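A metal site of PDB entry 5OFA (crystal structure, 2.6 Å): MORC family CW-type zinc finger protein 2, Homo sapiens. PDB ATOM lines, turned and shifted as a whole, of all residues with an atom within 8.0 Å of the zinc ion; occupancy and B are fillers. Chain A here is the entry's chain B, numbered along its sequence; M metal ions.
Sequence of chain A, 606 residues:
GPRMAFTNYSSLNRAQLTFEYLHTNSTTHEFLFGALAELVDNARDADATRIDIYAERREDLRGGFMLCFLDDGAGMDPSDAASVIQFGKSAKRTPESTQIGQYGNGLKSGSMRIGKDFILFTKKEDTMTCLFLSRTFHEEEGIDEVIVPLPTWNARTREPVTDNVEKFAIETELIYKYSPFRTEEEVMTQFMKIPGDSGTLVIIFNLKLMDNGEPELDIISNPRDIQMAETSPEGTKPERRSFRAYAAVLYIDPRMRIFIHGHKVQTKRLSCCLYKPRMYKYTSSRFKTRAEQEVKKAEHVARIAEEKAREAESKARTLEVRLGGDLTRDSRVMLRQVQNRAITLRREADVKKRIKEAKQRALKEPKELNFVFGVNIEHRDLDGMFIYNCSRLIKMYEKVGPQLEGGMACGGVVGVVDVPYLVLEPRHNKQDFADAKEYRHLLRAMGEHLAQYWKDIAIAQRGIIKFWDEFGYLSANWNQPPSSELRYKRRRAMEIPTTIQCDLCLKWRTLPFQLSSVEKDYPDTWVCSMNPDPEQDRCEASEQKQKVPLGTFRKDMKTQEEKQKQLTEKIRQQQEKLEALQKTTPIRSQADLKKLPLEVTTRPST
The zinc ion is bound by SG of Cys 528 (1.9 Å), SG of Cys 502 (2.0 Å), SG of Cys 505 (2.5 Å) and SG of Cys 539 (2.7 Å).
The zinc ion has four donor atoms within binding distance.
Four residues have an atom within 4 Å of the zinc ion: Cys 502, Cys 505, Cys 528 and Cys 539.
NE of Arg 509 lies close to SG of Cys 528 (3.5 Å).
The backbone NH (N) of Leu 504 sits close to the side-chain sulfur (SG) of Cys 502.
O of Lys 507 is in hydrogen-bond range of N of Cys 502 (2.8 Å).
The side-chain sulfur of Cys 505 sits close to the backbone NH of Lys 507, 3.8 Å away.
O of Cys 539 lies within hydrogen-bond range of NH2 of Arg 509 (3.4 Å).
The backbone carbonyl oxygen (O) of Cys 539 is in hydrogen-bond range of the side-chain amino group (NZ) of Lys 507, at 2.7 Å.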
ATOM      1  N   GLN A 501     -26.517  24.561  -7.956  1.00  0.00           N
ATOM      2  CA  GLN A 501     -26.384  23.170  -7.557  1.00  0.00           C
ATOM      3  C   GLN A 501     -27.616  22.370  -8.014  1.00  0.00           C
ATOM      4  O   GLN A 501     -28.751  22.807  -7.865  1.00  0.00           O
ATOM      5  CB  GLN A 501     -26.162  23.076  -6.044  1.00  0.00           C
ATOM      6  CG  GLN A 501     -26.020  21.666  -5.567  1.00  0.00           C
ATOM      7  CD  GLN A 501     -25.770  21.495  -4.077  1.00  0.00           C
ATOM      8  OE1 GLN A 501     -26.080  22.394  -3.330  1.00  0.00           O
ATOM      9  NE2 GLN A 501     -25.242  20.429  -3.646  1.00  0.00           N
ATOM     10  N   CYS A 502     -27.375  21.186  -8.558  1.00  0.00           N
ATOM     11  CA  CYS A 502     -28.495  20.358  -9.006  1.00  0.00           C
ATOM     12  C   CYS A 502     -29.155  19.729  -7.804  1.00  0.00           C
ATOM     13  O   CYS A 502     -28.490  19.113  -6.987  1.00  0.00           O
ATOM     14  CB  CYS A 502     -28.050  19.242  -9.974  1.00  0.00           C
ATOM     15  SG  CYS A 502     -29.352  18.016 -10.509  1.00  0.00           S
ATOM     16  N   ASP A 503     -30.476  19.879  -7.728  1.00  0.00           N
ATOM     17  CA  ASP A 503     -31.238  19.300  -6.636  1.00  0.00           C
ATOM     18  C   ASP A 503     -31.235  17.804  -6.564  1.00  0.00           C
ATOM     19  O   ASP A 503     -31.384  17.259  -5.489  1.00  0.00           O
ATOM     20  CB  ASP A 503     -32.682  19.761  -6.626  1.00  0.00           C
ATOM     21  CG  ASP A 503     -33.008  20.639  -5.450  1.00  0.00           C
ATOM     22  OD1 ASP A 503     -32.982  20.261  -4.212  1.00  0.00           O
ATOM     23  OD2 ASP A 503     -33.205  21.841  -5.860  1.00  0.00           O
ATOM     24  N   LEU A 504     -31.070  17.151  -7.708  1.00  0.00           N
ATOM     25  CA  LEU A 504     -30.972  15.674  -7.802  1.00  0.00           C
ATOM     26  C   LEU A 504     -29.600  15.100  -7.456  1.00  0.00           C
ATOM     27  O   LEU A 504     -29.487  14.301  -6.556  1.00  0.00           O
ATOM     28  CB  LEU A 504     -31.372  15.185  -9.210  1.00  0.00           C
ATOM     29  CG  LEU A 504     -32.839  15.378  -9.635  1.00  0.00           C
ATOM     30  CD1 LEU A 504     -33.078  14.994 -11.078  1.00  0.00           C
ATOM     31  CD2 LEU A 504     -33.769  14.564  -8.736  1.00  0.00           C
ATOM     32  N   CYS A 505     -28.559  15.495  -8.177  1.00  0.00           N
ATOM     33  CA  CYS A 505     -27.251  14.869  -8.020  1.00  0.00           C
ATOM     34  C   CYS A 505     -26.286  15.639  -7.093  1.00  0.00           C
ATOM     35  O   CYS A 505     -25.203  15.131  -6.823  1.00  0.00           O
ATOM     36  CB  CYS A 505     -26.627  14.546  -9.407  1.00  0.00           C
ATOM     37  SG  CYS A 505     -26.172  15.938 -10.384  1.00  0.00           S
ATOM     38  N   LEU A 506     -26.681  16.839  -6.623  1.00  0.00           N
ATOM     39  CA  LEU A 506     -25.804  17.706  -5.783  1.00  0.00           C
ATOM     40  C   LEU A 506     -24.537  18.207  -6.448  1.00  0.00           C
ATOM     41  O   LEU A 506     -23.670  18.756  -5.776  1.00  0.00           O
ATOM     42  CB  LEU A 506     -25.463  17.028  -4.439  1.00  0.00           C
ATOM     43  CG  LEU A 506     -26.661  16.634  -3.619  1.00  0.00           C
ATOM     44  CD1 LEU A 506     -26.177  16.350  -2.213  1.00  0.00           C
ATOM     45  CD2 LEU A 506     -27.724  17.724  -3.591  1.00  0.00           C
ATOM     46  N   LYS A 507     -24.425  18.055  -7.771  1.00  0.00           N
ATOM     47  CA  LYS A 507     -23.309  18.669  -8.489  1.00  0.00           C
ATOM     48  C   LYS A 507     -23.505  20.168  -8.682  1.00  0.00           C
ATOM     49  O   LYS A 507     -24.636  20.648  -8.804  1.00  0.00           O
ATOM     50  CB  LYS A 507     -23.125  18.016  -9.851  1.00  0.00           C
ATOM     51  CG  LYS A 507     -22.766  16.547  -9.784  1.00  0.00           C
ATOM     52  CD  LYS A 507     -22.489  16.051 -11.194  1.00  0.00           C
ATOM     53  CE  LYS A 507     -21.979  14.639 -11.218  1.00  0.00           C
ATOM     54  NZ  LYS A 507     -23.013  13.699 -10.948  1.00  0.00           N
ATOM     55  N   TRP A 508     -22.402  20.892  -8.713  1.00  0.00           N
ATOM     56  CA  TRP A 508     -22.374  22.336  -8.939  1.00  0.00           C
ATOM     57  C   TRP A 508     -22.111  22.563 -10.437  1.00  0.00           C
ATOM     58  O   TRP A 508     -21.220  21.924 -11.038  1.00  0.00           O
ATOM     59  CB  TRP A 508     -21.286  23.021  -8.094  1.00  0.00           C
ATOM     60  CG  TRP A 508     -21.716  23.169  -6.688  1.00  0.00           C
ATOM     61  CD1 TRP A 508     -21.452  22.330  -5.676  1.00  0.00           C
ATOM     62  CD2 TRP A 508     -22.471  24.242  -6.132  1.00  0.00           C
ATOM     63  NE1 TRP A 508     -22.042  22.790  -4.513  1.00  0.00           N
ATOM     64  CE2 TRP A 508     -22.661  23.966  -4.764  1.00  0.00           C
ATOM     65  CE3 TRP A 508     -23.025  25.388  -6.642  1.00  0.00           C
ATOM     66  CZ2 TRP A 508     -23.371  24.821  -3.924  1.00  0.00           C
ATOM     67  CZ3 TRP A 508     -23.762  26.222  -5.779  1.00  0.00           C
ATOM     68  CH2 TRP A 508     -23.908  25.939  -4.450  1.00  0.00           C
ATOM     69  N   ARG A 509     -22.876  23.466 -11.011  1.00  0.00           N
ATOM     70  CA  ARG A 509     -22.757  23.809 -12.430  1.00  0.00           C
ATOM     71  C   ARG A 509     -22.700  25.305 -12.635  1.00  0.00           C
ATOM     72  O   ARG A 509     -23.209  26.083 -11.837  1.00  0.00           O
ATOM     73  CB  ARG A 509     -23.913  23.243 -13.270  1.00  0.00           C
ATOM     74  CG  ARG A 509     -24.267  21.779 -13.012  1.00  0.00           C
ATOM     75  CD  ARG A 509     -23.186  20.797 -13.480  1.00  0.00           C
ATOM     76  NE  ARG A 509     -23.750  19.482 -13.772  1.00  0.00           N
ATOM     77  CZ  ARG A 509     -23.042  18.372 -13.957  1.00  0.00           C
ATOM     78  NH1 ARG A 509     -21.729  18.395 -13.909  1.00  0.00           N
ATOM     79  NH2 ARG A 509     -23.664  17.225 -14.240  1.00  0.00           N
ATOM     80  N   TRP A 526     -33.799  23.445  -9.158  1.00  0.00           N
ATOM     81  CA  TRP A 526     -33.106  23.524 -10.429  1.00  0.00           C
ATOM     82  C   TRP A 526     -32.365  22.200 -10.593  1.00  0.00           C
ATOM     83  O   TRP A 526     -31.797  21.665  -9.617  1.00  0.00           O
ATOM     84  CB  TRP A 526     -32.124  24.708 -10.457  1.00  0.00           C
ATOM     85  CG  TRP A 526     -31.429  24.877 -11.800  1.00  0.00           C
ATOM     86  CD1 TRP A 526     -31.797  25.707 -12.806  1.00  0.00           C
ATOM     87  CD2 TRP A 526     -30.243  24.220 -12.238  1.00  0.00           C
ATOM     88  NE1 TRP A 526     -30.911  25.603 -13.844  1.00  0.00           N
ATOM     89  CE2 TRP A 526     -29.946  24.697 -13.519  1.00  0.00           C
ATOM     90  CE3 TRP A 526     -29.382  23.285 -11.663  1.00  0.00           C
ATOM     91  CZ2 TRP A 526     -28.853  24.258 -14.263  1.00  0.00           C
ATOM     92  CZ3 TRP A 526     -28.295  22.848 -12.386  1.00  0.00           C
ATOM     93  CH2 TRP A 526     -28.041  23.333 -13.679  1.00  0.00           C
ATOM     94  N   VAL A 527     -32.367  21.679 -11.796  1.00  0.00           N
ATOM     95  CA  VAL A 527     -31.658  20.428 -12.049  1.00  0.00           C
ATOM     96  C   VAL A 527     -30.794  20.583 -13.299  1.00  0.00           C
ATOM     97  O   VAL A 527     -30.971  21.507 -14.132  1.00  0.00           O
ATOM     98  CB  VAL A 527     -32.611  19.225 -12.150  1.00  0.00           C
ATOM     99  CG1 VAL A 527     -33.374  19.065 -10.835  1.00  0.00           C
ATOM    100  CG2 VAL A 527     -33.578  19.388 -13.336  1.00  0.00           C
ATOM    101  N   CYS A 528     -29.843  19.668 -13.431  1.00  0.00           N
ATOM    102  CA  CYS A 528     -28.859  19.740 -14.476  1.00  0.00           C
ATOM    103  C   CYS A 528     -29.433  19.889 -15.872  1.00  0.00           C
ATOM    104  O   CYS A 528     -28.814  20.543 -16.697  1.00  0.00           O
ATOM    105  CB  CYS A 528     -27.990  18.506 -14.488  1.00  0.00           C
ATOM    106  SG  CYS A 528     -26.959  18.182 -12.994  1.00  0.00           S
ATOM    107  N   SER A 529     -30.603  19.283 -16.133  1.00  0.00           N
ATOM    108  CA  SER A 529     -31.191  19.292 -17.462  1.00  0.00           C
ATOM    109  C   SER A 529     -31.847  20.598 -17.794  1.00  0.00           C
ATOM    110  O   SER A 529     -32.260  20.772 -18.909  1.00  0.00           O
ATOM    111  CB  SER A 529     -32.162  18.134 -17.637  1.00  0.00           C
ATOM    112  OG  SER A 529     -33.351  18.386 -16.908  1.00  0.00           O
ATOM    113  N   MET A 530     -31.934  21.520 -16.836  1.00  0.00           N
ATOM    114  CA  MET A 530     -32.345  22.900 -17.109  1.00  0.00           C
ATOM    115  C   MET A 530     -31.154  23.759 -17.669  1.00  0.00           C
ATOM    116  O   MET A 530     -31.361  24.788 -18.342  1.00  0.00           O
ATOM    117  CB  MET A 530     -33.002  23.496 -15.858  1.00  0.00           C
ATOM    118  CG  MET A 530     -34.029  22.600 -15.136  1.00  0.00           C
ATOM    119  SD  MET A 530     -34.876  23.533 -13.855  1.00  0.00           S
ATOM    120  CE  MET A 530     -35.923  22.296 -13.148  1.00  0.00           C
ATOM    121  N   GLN A 536     -22.805  20.351 -19.810  1.00  0.00           N
ATOM    122  CA  GLN A 536     -23.158  20.070 -18.416  1.00  0.00           C
ATOM    123  C   GLN A 536     -24.670  19.886 -18.234  1.00  0.00           C
ATOM    124  O   GLN A 536     -25.209  20.261 -17.172  1.00  0.00           O
ATOM    125  CB  GLN A 536     -22.712  21.238 -17.499  1.00  0.00           C
ATOM    126  CG  GLN A 536     -21.243  21.660 -17.391  1.00  0.00           C
ATOM    127  CD  GLN A 536     -21.083  22.994 -16.591  1.00  0.00           C
ATOM    128  OE1 GLN A 536     -21.799  23.971 -16.838  1.00  0.00           O
ATOM    129  NE2 GLN A 536     -20.159  23.023 -15.631  1.00  0.00           N
ATOM    130  N   ASP A 537     -25.381  19.345 -19.228  1.00  0.00           N
ATOM    131  CA  ASP A 537     -26.887  19.305 -19.153  1.00  0.00           C
ATOM    132  C   ASP A 537     -27.552  18.002 -18.610  1.00  0.00           C
ATOM    133  O   ASP A 537     -28.762  17.812 -18.663  1.00  0.00           O
ATOM    134  CB  ASP A 537     -27.541  19.759 -20.461  1.00  0.00           C
ATOM    135  CG  ASP A 537     -27.096  18.960 -21.658  1.00  0.00           C
ATOM    136  OD1 ASP A 537     -26.299  17.995 -21.525  1.00  0.00           O
ATOM    137  OD2 ASP A 537     -27.562  19.334 -22.761  1.00  0.00           O
ATOM    138  N   ARG A 538     -26.754  17.128 -18.038  1.00  0.00           N
ATOM    139  CA  ARG A 538     -27.274  15.872 -17.534  1.00  0.00           C
ATOM    140  C   ARG A 538     -26.535  15.587 -16.232  1.00  0.00           C
ATOM    141  O   ARG A 538     -25.401  16.004 -16.058  1.00  0.00           O
ATOM    142  CB  ARG A 538     -27.112  14.766 -18.597  1.00  0.00           C
ATOM    143  CG  ARG A 538     -25.988  15.037 -19.602  1.00  0.00           C
ATOM    144  CD  ARG A 538     -25.825  13.953 -20.652  1.00  0.00           C
ATOM    145  NE  ARG A 538     -24.618  13.139 -20.427  1.00  0.00           N
ATOM    146  CZ  ARG A 538     -23.367  13.500 -20.729  1.00  0.00           C
ATOM    147  NH1 ARG A 538     -23.106  14.709 -21.256  1.00  0.00           N
ATOM    148  NH2 ARG A 538     -22.352  12.662 -20.465  1.00  0.00           N
ATOM    149  N   CYS A 539     -27.197  14.893 -15.313  1.00  0.00           N
ATOM    150  CA  CYS A 539     -26.640  14.668 -13.993  1.00  0.00           C
ATOM    151  C   CYS A 539     -25.314  13.901 -14.080  1.00  0.00           C
ATOM    152  O   CYS A 539     -24.412  14.076 -13.211  1.00  0.00           O
ATOM    153  CB  CYS A 539     -27.651  13.956 -13.109  1.00  0.00           C
ATOM    154  SG  CYS A 539     -29.149  15.004 -12.900  1.00  0.00           S
ATOM    155  N   GLU A 540     -25.272  13.092 -15.169  1.00  0.00           N
ATOM    156  CA  GLU A 540     -24.134  12.272 -15.649  1.00  0.00           C
ATOM    157  C   GLU A 540     -22.868  13.015 -16.092  1.00  0.00           C
ATOM    158  O   GLU A 540     -21.809  12.399 -16.127  1.00  0.00           O
ATOM    159  CB  GLU A 540     -24.558  11.369 -16.845  1.00  0.00           C
ATOM    160  CG  GLU A 540     -25.525  10.211 -16.540  1.00  0.00           C
ATOM    161  CD  GLU A 540     -27.016  10.556 -16.668  1.00  0.00           C
ATOM    162  OE1 GLU A 540     -27.425  11.346 -17.580  1.00  0.00           O
ATOM    163  OE2 GLU A 540     -27.785  10.012 -15.826  1.00  0.00           O
ATOM    164  N   ALA A 541     -22.960  14.299 -16.450  1.00  0.00           N
ATOM    165  CA  ALA A 541     -21.799  15.048 -16.926  1.00  0.00           C
ATOM    166  C   ALA A 541     -20.948  15.320 -15.721  1.00  0.00           C
ATOM    167  O   ALA A 541     -21.426  15.846 -14.733  1.00  0.00           O
ATOM    168  CB  ALA A 541     -22.226  16.331 -17.635  1.00  0.00           C
HETATM  169 ZN    ZN M   1     -27.966  17.145 -11.689  1.00  0.00          ZN
